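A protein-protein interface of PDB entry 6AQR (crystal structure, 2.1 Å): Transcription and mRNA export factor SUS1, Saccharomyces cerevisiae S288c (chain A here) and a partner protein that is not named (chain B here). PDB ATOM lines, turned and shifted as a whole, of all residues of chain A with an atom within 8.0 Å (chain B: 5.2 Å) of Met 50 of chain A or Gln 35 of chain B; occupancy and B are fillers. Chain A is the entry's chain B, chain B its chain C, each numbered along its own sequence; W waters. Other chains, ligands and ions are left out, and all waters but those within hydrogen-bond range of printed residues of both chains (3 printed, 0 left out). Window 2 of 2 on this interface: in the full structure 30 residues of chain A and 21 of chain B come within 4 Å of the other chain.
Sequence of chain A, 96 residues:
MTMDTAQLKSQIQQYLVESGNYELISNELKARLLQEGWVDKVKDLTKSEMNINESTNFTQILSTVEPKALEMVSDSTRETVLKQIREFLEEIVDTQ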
ATOM      1  N   VAL A  42      -4.842   5.171   5.264  1.00  0.00           N
ATOM      2  CA  VAL A  42      -4.389   6.565   5.100  1.00  0.00           C
ATOM      3  C   VAL A  42      -5.566   7.490   4.664  1.00  0.00           C
ATOM      4  O   VAL A  42      -5.705   8.593   5.178  1.00  0.00           O
ATOM      5  CB  VAL A  42      -3.167   6.645   4.159  1.00  0.00           C
ATOM      6  CG1 VAL A  42      -2.757   8.079   3.867  1.00  0.00           C
ATOM      7  CG2 VAL A  42      -1.990   5.893   4.786  1.00  0.00           C
ATOM      8  N   LYS A  43      -6.446   7.001   3.790  1.00  0.00           N
ATOM      9  CA  LYS A  43      -7.633   7.701   3.388  1.00  0.00           C
ATOM     10  C   LYS A  43      -8.554   7.970   4.561  1.00  0.00           C
ATOM     11  O   LYS A  43      -9.024   9.089   4.684  1.00  0.00           O
ATOM     12  CB  LYS A  43      -8.396   6.931   2.312  1.00  0.00           C
ATOM     13  CG  LYS A  43      -7.710   6.980   0.947  1.00  0.00           C
ATOM     14  CD  LYS A  43      -8.605   6.353  -0.108  1.00  0.00           C
ATOM     15  CE  LYS A  43      -7.888   6.149  -1.444  1.00  0.00           C
ATOM     16  NZ  LYS A  43      -9.024   6.048  -2.406  1.00  0.00           N
ATOM     17  N   ASP A  44      -8.808   6.958   5.400  1.00  0.00           N
ATOM     18  CA  ASP A  44      -9.574   7.109   6.654  1.00  0.00           C
ATOM     19  C   ASP A  44      -8.955   8.088   7.665  1.00  0.00           C
ATOM     20  O   ASP A  44      -9.661   8.930   8.211  1.00  0.00           O
ATOM     21  CB  ASP A  44      -9.785   5.774   7.321  1.00  0.00           C
ATOM     22  CG  ASP A  44     -10.724   4.876   6.526  1.00  0.00           C
ATOM     23  OD1 ASP A  44     -11.139   5.238   5.385  1.00  0.00           O
ATOM     24  OD2 ASP A  44     -11.074   3.800   7.061  1.00  0.00           O
ATOM     25  N   LEU A  45      -7.644   8.005   7.844  1.00  0.00           N
ATOM     26  CA  LEU A  45      -6.885   8.947   8.664  1.00  0.00           C
ATOM     27  C   LEU A  45      -7.021  10.405   8.158  1.00  0.00           C
ATOM     28  O   LEU A  45      -7.266  11.327   8.958  1.00  0.00           O
ATOM     29  CB  LEU A  45      -5.411   8.512   8.739  1.00  0.00           C
ATOM     30  CG  LEU A  45      -4.338   9.392   9.415  1.00  0.00           C
ATOM     31  CD1 LEU A  45      -4.692   9.687  10.867  1.00  0.00           C
ATOM     32  CD2 LEU A  45      -2.949   8.716   9.329  1.00  0.00           C
ATOM     33  N   THR A  46      -6.859  10.599   6.840  1.00  0.00           N
ATOM     34  CA  THR A  46      -6.922  11.928   6.252  1.00  0.00           C
ATOM     35  C   THR A  46      -8.313  12.502   6.433  1.00  0.00           C
ATOM     36  O   THR A  46      -8.439  13.708   6.756  1.00  0.00           O
ATOM     37  CB  THR A  46      -6.523  11.882   4.781  1.00  0.00           C
ATOM     38  OG1 THR A  46      -5.186  11.379   4.743  1.00  0.00           O
ATOM     39  CG2 THR A  46      -6.524  13.282   4.154  1.00  0.00           C
ATOM     40  N   LYS A  47      -9.335  11.670   6.289  1.00  0.00           N
ATOM     41  CA  LYS A  47     -10.720  12.116   6.459  1.00  0.00           C
ATOM     42  C   LYS A  47     -10.945  12.621   7.926  1.00  0.00           C
ATOM     43  O   LYS A  47     -11.510  13.673   8.164  1.00  0.00           O
ATOM     44  CB  LYS A  47     -11.692  10.987   6.052  1.00  0.00           C
ATOM     45  CG  LYS A  47     -13.190  11.222   6.249  1.00  0.00           C
ATOM     46  CD  LYS A  47     -14.007   9.983   5.802  1.00  0.00           C
ATOM     47  CE  LYS A  47     -15.369  10.274   5.159  1.00  0.00           C
ATOM     48  NZ  LYS A  47     -16.364  10.653   6.212  1.00  0.00           N
ATOM     49  N   SER A  48     -10.525  11.814   8.882  1.00  0.00           N
ATOM     50  CA  SER A  48     -10.582  12.162  10.277  1.00  0.00           C
ATOM     51  C   SER A  48      -9.744  13.438  10.620  1.00  0.00           C
ATOM     52  O   SER A  48     -10.242  14.358  11.314  1.00  0.00           O
ATOM     53  CB  SER A  48     -10.134  10.954  11.125  1.00  0.00           C
ATOM     54  OG  SER A  48      -9.966  11.374  12.460  1.00  0.00           O
ATOM     55  N   GLU A  49      -8.515  13.518  10.150  1.00  0.00           N
ATOM     56  CA  GLU A  49      -7.717  14.764  10.357  1.00  0.00           C
ATOM     57  C   GLU A  49      -8.371  16.030   9.786  1.00  0.00           C
ATOM     58  O   GLU A  49      -8.372  17.074  10.416  1.00  0.00           O
ATOM     59  CB  GLU A  49      -6.286  14.613   9.867  1.00  0.00           C
ATOM     60  CG  GLU A  49      -5.451  13.616  10.663  1.00  0.00           C
ATOM     61  CD  GLU A  49      -5.373  13.929  12.171  1.00  0.00           C
ATOM     62  OE1 GLU A  49      -5.797  13.039  12.952  1.00  0.00           O
ATOM     63  OE2 GLU A  49      -4.914  15.045  12.576  1.00  0.00           O
ATOM     64  N   MET A  50      -9.042  15.905   8.655  1.00  0.00           N
ATOM     65  CA  MET A  50      -9.759  17.051   8.049  1.00  0.00           C
ATOM     66  C   MET A  50     -10.938  17.459   8.924  1.00  0.00           C
ATOM     67  O   MET A  50     -11.185  18.655   9.144  1.00  0.00           O
ATOM     68  CB  MET A  50     -10.232  16.761   6.619  1.00  0.00           C
ATOM     69  CG  MET A  50      -9.085  16.716   5.610  1.00  0.00           C
ATOM     70  SD  MET A  50      -9.626  16.597   3.889  1.00  0.00           S
ATOM     71  CE  MET A  50     -10.241  14.878   3.794  1.00  0.00           C
ATOM     72  N   ASN A  51     -11.668  16.471   9.401  1.00  0.00           N
ATOM     73  CA  ASN A  51     -12.734  16.735  10.305  1.00  0.00           C
ATOM     74  C   ASN A  51     -12.287  17.533  11.575  1.00  0.00           C
ATOM     75  O   ASN A  51     -12.854  18.585  11.867  1.00  0.00           O
ATOM     76  CB  ASN A  51     -13.443  15.439  10.681  1.00  0.00           C
ATOM     77  CG  ASN A  51     -14.745  15.714  11.351  1.00  0.00           C
ATOM     78  OD1 ASN A  51     -15.774  15.656  10.728  1.00  0.00           O
ATOM     79  ND2 ASN A  51     -14.701  16.098  12.591  1.00  0.00           N
ATOM     80  N   ILE A  52     -11.265  17.035  12.273  1.00  0.00           N
ATOM     81  CA  ILE A  52     -10.677  17.654  13.437  1.00  0.00           C
ATOM     82  C   ILE A  52     -10.156  19.055  13.106  1.00  0.00           C
ATOM     83  O   ILE A  52     -10.456  20.012  13.800  1.00  0.00           O
ATOM     84  CB  ILE A  52      -9.492  16.811  13.993  1.00  0.00           C
ATOM     85  CG1 ILE A  52      -9.986  15.511  14.627  1.00  0.00           C
ATOM     86  CG2 ILE A  52      -8.656  17.641  14.969  1.00  0.00           C
ATOM     87  CD1 ILE A  52      -8.853  14.482  14.729  1.00  0.00           C
ATOM     88  N   ASN A  53      -9.340  19.157  12.057  1.00  0.00           N
ATOM     89  CA  ASN A  53      -8.756  20.431  11.653  1.00  0.00           C
ATOM     90  C   ASN A  53      -9.770  21.506  11.192  1.00  0.00           C
ATOM     91  O   ASN A  53      -9.414  22.692  11.124  1.00  0.00           O
ATOM     92  CB  ASN A  53      -7.697  20.214  10.553  1.00  0.00           C
ATOM     93  CG  ASN A  53      -6.782  21.412  10.380  1.00  0.00           C
ATOM     94  OD1 ASN A  53      -6.641  22.006   9.275  1.00  0.00           O
ATOM     95  ND2 ASN A  53      -6.172  21.800  11.476  1.00  0.00           N
ATOM     96  N   GLU A  54     -10.973  21.066  10.803  1.00  0.00           N
ATOM     97  CA  GLU A  54     -12.039  21.915  10.254  1.00  0.00           C
ATOM     98  C   GLU A  54     -11.579  22.765   9.068  1.00  0.00           C
ATOM     99  O   GLU A  54     -11.933  23.948   8.926  1.00  0.00           O
ATOM    100  CB  GLU A  54     -12.654  22.770  11.382  1.00  0.00           C
ATOM    101  CG  GLU A  54     -13.538  21.923  12.330  1.00  0.00           C
ATOM    102  CD  GLU A  54     -14.141  22.699  13.514  1.00  0.00           C
ATOM    103  OE1 GLU A  54     -14.074  23.967  13.571  1.00  0.00           O
ATOM    104  OE2 GLU A  54     -14.704  22.020  14.399  1.00  0.00           O
ATOM    105  N   SER A  55     -10.763  22.139   8.215  1.00  0.00           N
ATOM    106  CA  SER A  55     -10.093  22.804   7.105  1.00  0.00           C
ATOM    107  C   SER A  55      -9.420  21.710   6.278  1.00  0.00           C
ATOM    108  O   SER A  55      -8.930  20.726   6.839  1.00  0.00           O
ATOM    109  CB  SER A  55      -9.031  23.782   7.599  1.00  0.00           C
ATOM    110  OG  SER A  55      -8.263  24.285   6.504  1.00  0.00           O
ATOM    111  N   THR A  56      -9.381  21.918   4.977  1.00  0.00           N
ATOM    112  CA  THR A  56      -8.751  20.981   4.051  1.00  0.00           C
ATOM    113  C   THR A  56      -7.384  21.433   3.638  1.00  0.00           C
ATOM    114  O   THR A  56      -6.830  20.852   2.717  1.00  0.00           O
ATOM    115  CB  THR A  56      -9.611  20.779   2.781  1.00  0.00           C
ATOM    116  OG1 THR A  56      -9.757  22.030   2.137  1.00  0.00           O
ATOM    117  CG2 THR A  56     -10.987  20.283   3.144  1.00  0.00           C
ATOM    118  N   ASN A  57      -6.839  22.468   4.301  1.00  0.00           N
ATOM    119  CA  ASN A  57      -5.505  22.990   3.959  1.00  0.00           C
ATOM    120  C   ASN A  57      -4.416  21.890   3.937  1.00  0.00           C
ATOM    121  O   ASN A  57      -4.111  21.253   4.957  1.00  0.00           O
ATOM    122  CB  ASN A  57      -5.096  24.055   4.923  1.00  0.00           C
ATOM    123  CG  ASN A  57      -3.719  24.625   4.601  1.00  0.00           C
ATOM    124  OD1 ASN A  57      -2.685  24.026   4.884  1.00  0.00           O
ATOM    125  ND2 ASN A  57      -3.712  25.808   3.998  1.00  0.00           N
ATOM    126  N   PHE A  58      -3.819  21.674   2.756  1.00  0.00           N
ATOM    127  CA  PHE A  58      -2.943  20.517   2.572  1.00  0.00           C
ATOM    128  C   PHE A  58      -1.741  20.550   3.527  1.00  0.00           C
ATOM    129  O   PHE A  58      -1.334  19.511   4.048  1.00  0.00           O
ATOM    130  CB  PHE A  58      -2.463  20.425   1.132  1.00  0.00           C
ATOM    131  CG  PHE A  58      -1.444  19.324   0.918  1.00  0.00           C
ATOM    132  CD1 PHE A  58      -0.089  19.592   0.898  1.00  0.00           C
ATOM    133  CD2 PHE A  58      -1.891  17.984   0.713  1.00  0.00           C
ATOM    134  CE1 PHE A  58       0.816  18.559   0.679  1.00  0.00           C
ATOM    135  CE2 PHE A  58      -0.998  16.958   0.517  1.00  0.00           C
ATOM    136  CZ  PHE A  58       0.347  17.235   0.490  1.00  0.00           C
ATOM    137  N   ILE A  61      -2.971  19.537   7.059  1.00  0.00           N
ATOM    138  CA  ILE A  61      -3.394  18.092   7.100  1.00  0.00           C
ATOM    139  C   ILE A  61      -2.191  17.154   6.983  1.00  0.00           C
ATOM    140  O   ILE A  61      -2.123  16.210   7.733  1.00  0.00           O
ATOM    141  CB  ILE A  61      -4.415  17.806   5.994  1.00  0.00           C
ATOM    142  CG1 ILE A  61      -5.645  18.738   6.192  1.00  0.00           C
ATOM    143  CG2 ILE A  61      -4.769  16.303   5.932  1.00  0.00           C
ATOM    144  CD1 ILE A  61      -6.275  18.610   7.577  1.00  0.00           C
ATOM    145  N   LEU A  62      -1.265  17.440   6.037  1.00  0.00           N
ATOM    146  CA  LEU A  62      -0.069  16.599   5.808  1.00  0.00           C
ATOM    147  C   LEU A  62       0.839  16.533   7.044  1.00  0.00           C
ATOM    148  O   LEU A  62       1.279  15.428   7.465  1.00  0.00           O
ATOM    149  CB  LEU A  62       0.720  17.085   4.583  1.00  0.00           C
ATOM    150  CG  LEU A  62       1.978  16.222   4.369  1.00  0.00           C
ATOM    151  CD1 LEU A  62       1.543  14.843   3.845  1.00  0.00           C
ATOM    152  CD2 LEU A  62       2.923  16.931   3.426  1.00  0.00           C
ATOM    153  N   THR A  64      -0.005  16.537  10.079  1.00  0.00           N
ATOM    154  CA  THR A  64      -0.512  15.555  11.073  1.00  0.00           C
ATOM    155  C   THR A  64      -0.656  14.100  10.544  1.00  0.00           C
ATOM    156  O   THR A  64      -0.376  13.113  11.272  1.00  0.00           O
ATOM    157  CB  THR A  64      -1.795  16.029  11.849  1.00  0.00           C
ATOM    158  OG1 THR A  64      -2.927  16.042  10.983  1.00  0.00           O
ATOM    159  CG2 THR A  64      -1.607  17.465  12.508  1.00  0.00           C
ATOM    160  N   VAL A  65      -1.083  13.963   9.291  1.00  0.00           N
ATOM    161  CA  VAL A  65      -1.209  12.607   8.679  1.00  0.00           C
ATOM    162  C   VAL A  65       0.134  11.920   8.485  1.00  0.00           C
ATOM    163  O   VAL A  65       0.288  10.740   8.822  1.00  0.00           O
ATOM    164  CB  VAL A  65      -2.017  12.655   7.364  1.00  0.00           C
ATOM    165  CG1 VAL A  65      -2.035  11.296   6.607  1.00  0.00           C
ATOM    166  CG2 VAL A  65      -3.416  13.127   7.700  1.00  0.00           C
ATOM    167  N   GLU B  31      -7.169  13.408  -1.450  1.00  0.00           N
ATOM    168  CA  GLU B  31      -8.312  13.528  -0.479  1.00  0.00           C
ATOM    169  C   GLU B  31      -8.619  14.988  -0.075  1.00  0.00           C
ATOM    170  O   GLU B  31      -9.787  15.334   0.099  1.00  0.00           O
ATOM    171  CB  GLU B  31      -8.054  12.755   0.822  1.00  0.00           C
ATOM    172  CG  GLU B  31      -7.773  11.269   0.633  1.00  0.00           C
ATOM    173  CD  GLU B  31      -8.967  10.543  -0.003  1.00  0.00           C
ATOM    174  OE1 GLU B  31      -8.900  10.174  -1.201  1.00  0.00           O
ATOM    175  OE2 GLU B  31     -10.010  10.346   0.666  1.00  0.00           O
ATOM    176  N   THR B  32      -7.597  15.824   0.095  1.00  0.00           N
ATOM    177  CA  THR B  32      -7.885  17.185   0.510  1.00  0.00           C
ATOM    178  C   THR B  32      -8.459  18.041  -0.613  1.00  0.00           C
ATOM    179  O   THR B  32      -9.355  18.815  -0.333  1.00  0.00           O
ATOM    180  CB  THR B  32      -6.670  17.917   1.094  1.00  0.00           C
ATOM    181  OG1 THR B  32      -5.615  17.969   0.127  1.00  0.00           O
ATOM    182  CG2 THR B  32      -6.237  17.270   2.406  1.00  0.00           C
ATOM    183  N   THR B  33      -7.942  17.933  -1.857  1.00  0.00           N
ATOM    184  CA  THR B  33      -8.603  18.627  -2.992  1.00  0.00           C
ATOM    185  C   THR B  33     -10.039  18.200  -3.169  1.00  0.00           C
ATOM    186  O   THR B  33     -10.911  19.000  -3.389  1.00  0.00           O
ATOM    187  CB  THR B  33      -7.842  18.456  -4.340  1.00  0.00           C
ATOM    188  OG1 THR B  33      -7.710  17.045  -4.653  1.00  0.00           O
ATOM    189  CG2 THR B  33      -6.456  19.095  -4.200  1.00  0.00           C
ATOM    190  N   GLN B  34     -10.309  16.903  -3.036  1.00  0.00           N
ATOM    191  CA  GLN B  34     -11.651  16.424  -3.147  1.00  0.00           C
ATOM    192  C   GLN B  34     -12.626  17.044  -2.127  1.00  0.00           C
ATOM    193  O   GLN B  34     -13.721  17.484  -2.508  1.00  0.00           O
ATOM    194  CB  GLN B  34     -11.683  14.888  -3.078  1.00  0.00           C
ATOM    195  CG  GLN B  34     -11.437  14.190  -4.402  1.00  0.00           C
ATOM    196  CD  GLN B  34     -10.922  12.732  -4.233  1.00  0.00           C
ATOM    197  OE1 GLN B  34     -11.357  11.986  -3.360  1.00  0.00           O
ATOM    198  NE2 GLN B  34      -9.935  12.374  -5.051  1.00  0.00           N
ATOM    199  N   GLN B  35     -12.253  17.043  -0.862  1.00  0.00           N
ATOM    200  CA  GLN B  35     -13.096  17.630   0.187  1.00  0.00           C
ATOM    201  C   GLN B  35     -13.105  19.183   0.055  1.00  0.00           C
ATOM    202  O   GLN B  35     -14.116  19.806   0.333  1.00  0.00           O
ATOM    203  CB  GLN B  35     -12.565  17.233   1.555  1.00  0.00           C
ATOM    204  CG  GLN B  35     -13.460  17.619   2.739  1.00  0.00           C
ATOM    205  CD  GLN B  35     -14.785  16.876   2.771  1.00  0.00           C
ATOM    206  OE1 GLN B  35     -15.158  16.233   1.827  1.00  0.00           O
ATOM    207  NE2 GLN B  35     -15.505  16.983   3.871  1.00  0.00           N
ATOM    208  N   GLN B  36     -11.983  19.786  -0.364  1.00  0.00           N
ATOM    209  CA  GLN B  36     -12.009  21.214  -0.676  1.00  0.00           C
ATOM    210  C   GLN B  36     -13.104  21.542  -1.671  1.00  0.00           C
ATOM    211  O   GLN B  36     -13.901  22.455  -1.432  1.00  0.00           O
ATOM    212  CB  GLN B  36     -10.654  21.747  -1.202  1.00  0.00           C
ATOM    213  CG  GLN B  36     -10.669  23.278  -1.256  1.00  0.00           C
ATOM    214  CD  GLN B  36      -9.457  23.881  -1.948  1.00  0.00           C
ATOM    215  OE1 GLN B  36      -8.923  23.335  -2.903  1.00  0.00           O
ATOM    216  NE2 GLN B  36      -9.019  25.045  -1.448  1.00  0.00           N
ATOM    217  N   LEU B  37     -13.142  20.822  -2.806  1.00  0.00           N
ATOM    218  CA  LEU B  37     -14.153  21.046  -3.791  1.00  0.00           C
ATOM    219  C   LEU B  37     -15.545  20.878  -3.187  1.00  0.00           C
ATOM    220  O   LEU B  37     -16.438  21.640  -3.501  1.00  0.00           O
ATOM    221  CB  LEU B  37     -14.000  20.045  -4.997  1.00  0.00           C
ATOM    222  CG  LEU B  37     -15.097  20.148  -6.103  1.00  0.00           C
ATOM    223  CD1 LEU B  37     -15.205  21.506  -6.856  1.00  0.00           C
ATOM    224  CD2 LEU B  37     -14.852  19.035  -7.136  1.00  0.00           C
ATOM    225  N   LEU B  38     -15.757  19.839  -2.373  1.00  0.00           N
ATOM    226  CA  LEU B  38     -17.116  19.575  -1.853  1.00  0.00           C
ATOM    227  C   LEU B  38     -17.570  20.733  -0.892  1.00  0.00           C
ATOM    228  O   LEU B  38     -18.744  21.170  -0.943  1.00  0.00           O
ATOM    229  CB  LEU B  38     -17.197  18.264  -1.095  1.00  0.00           C
ATOM    230  CG  LEU B  38     -17.110  16.956  -1.931  1.00  0.00           C
ATOM    231  CD1 LEU B  38     -17.415  15.749  -1.048  1.00  0.00           C
ATOM    232  CD2 LEU B  38     -17.972  16.996  -3.194  1.00  0.00           C
ATOM    233  N   LYS B  39     -16.630  21.210  -0.067  1.00  0.00           N
ATOM    234  CA  LYS B  39     -16.942  22.238   0.957  1.00  0.00           C
ATOM    235  C   LYS B  39     -17.261  23.531   0.248  1.00  0.00           C
ATOM    236  O   LYS B  39     -18.260  24.137   0.543  1.00  0.00           O
ATOM    237  CB  LYS B  39     -15.790  22.442   1.921  1.00  0.00           C
ATOM    238  CG  LYS B  39     -15.544  21.307   2.903  1.00  0.00           C
ATOM    239  CD  LYS B  39     -16.748  20.990   3.752  1.00  0.00           C
ATOM    240  CE  LYS B  39     -16.325  20.210   4.994  1.00  0.00           C
ATOM    241  NZ  LYS B  39     -16.705  20.888   6.274  1.00  0.00           N
ATOM    242  N   THR B  40     -16.460  23.908  -0.735  1.00  0.00           N
ATOM    243  CA  THR B  40     -16.770  25.106  -1.593  1.00  0.00           C
ATOM    244  C   THR B  40     -18.073  24.977  -2.374  1.00  0.00           C
ATOM    245  O   THR B  40     -18.869  25.911  -2.491  1.00  0.00           O
ATOM    246  CB  THR B  40     -15.649  25.361  -2.635  1.00  0.00           C
ATOM    247  OG1 THR B  40     -14.423  25.473  -1.956  1.00  0.00           O
ATOM    248  CG2 THR B  40     -15.861  26.671  -3.478  1.00  0.00           C
ATOM    249  N   LEU B  45     -22.771  21.366   3.151  1.00  0.00           N
ATOM    250  CA  LEU B  45     -22.336  19.957   3.145  1.00  0.00           C
ATOM    251  C   LEU B  45     -22.363  19.323   4.543  1.00  0.00           C
ATOM    252  O   LEU B  45     -21.705  19.804   5.461  1.00  0.00           O
ATOM    253  CB  LEU B  45     -20.909  19.820   2.522  1.00  0.00           C
ATOM    254  CG  LEU B  45     -20.363  18.384   2.457  1.00  0.00           C
ATOM    255  CD1 LEU B  45     -20.999  17.663   1.270  1.00  0.00           C
ATOM    256  CD2 LEU B  45     -18.863  18.291   2.381  1.00  0.00           C
HETATM  257  O   HOH W   1     -10.561   8.209  -2.877  1.00  0.00           O
HETATM  258  O   HOH W   2      -5.934  20.664  -0.369  1.00  0.00           O
HETATM  259  O   HOH W   3      -8.395  23.835   1.132  1.00  0.00           O
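The side-chain hydroxyl (OG1) of Thr 40 of chain B is in hydrogen-bond range of the backbone carbonyl oxygen (O) of Gln 36 of chain B, 3.1 Å away. OG1 of Thr 64 of chain A lies within hydrogen-bond range of O of Ile 61 of chain A (3.4 Å). The side-chain hydroxyl (OG1) of Thr 46 of chain A is in hydrogen-bond range of the backbone carbonyl oxygen (O) of Val 42 of chain A (2.9 Å).
Glu 31 of chain B touches Lys 43 of chain A (CD to CG, 3.9 Å). Thr 46 of chain A touches Glu 31 of chain B. Met 50 of chain A touches Glu 31 of chain B (CE to O, 3.8 Å). Thr 32 of chain B touches Met 50 of chain A (CG2 to SD, 3.8 Å). CB of Gln 35 of chain B touches SD of Met 50 of chain A, 3.8 Å away. O of Thr 56 of chain A touches CB of Thr 32 of chain B, 3.4 Å away. Gln 35 of chain B touches Thr 56 of chain A (CG to CG2, 3.7 Å). CB of Gln 36 of chain B touches OG1 of Thr 56 of chain A (3.5 Å). Phe 58 of chain A touches Thr 32 of chain B (CD2 to OG1, 3.8 Å). Ile 61 of chain A touches Thr 32 of chain B.
Val 42 of chain A touches none of the printed residues of chain B. Printed residues of chain B within 4 Å of Thr 46 of chain A: Glu 31 (3.7 Å). Met 50 of chain A touches just these residues of chain B: Glu 31, Thr 32 and Gln 35. Printed residues of chain B within 4 Å of Phe 58 of chain A: Thr 32. Printed residues of chain B within 4 Å of Ile 61 of chain A: Thr 32. Of the printed residues of chain A, Thr 32 of chain B touches Met 50, Thr 56, Phe 58 and Ile 61. Thr 33 of chain B touches none of the printed residues of chain A. Of the printed residues of chain A, Gln 36 of chain B touches Thr 56. The nearest printed residue of chain B that does not touch Met 50 of chain A is Gln 36 of chain B (5.8 Å).
Hydrophobic or aromatic side chains of chain A that line the printed part of chain B: Met 50, Phe 58 and Ile 61. Among the printed residues, no Asp or Glu carboxylate lies within 4 Å of a Lys or Arg side-chain nitrogen of the other chain.
Water W3 bridges OG1 of Thr 56 of chain A (2.5 Å) and NE2 of Gln 36 of chain B (2.9 Å). Water W1 lies within hydrogen-bond range of the side-chain amino group of Lys 43 of chain A (2.7 Å) and the side-chain carboxylate of Glu 31 of chain B (3.1 Å). Water W2 bridges the side-chain hydroxyl of Thr 32 of chain B (2.8 Å) and the backbone carbonyl oxygen of Thr 56 of chain A (3.2 Å).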
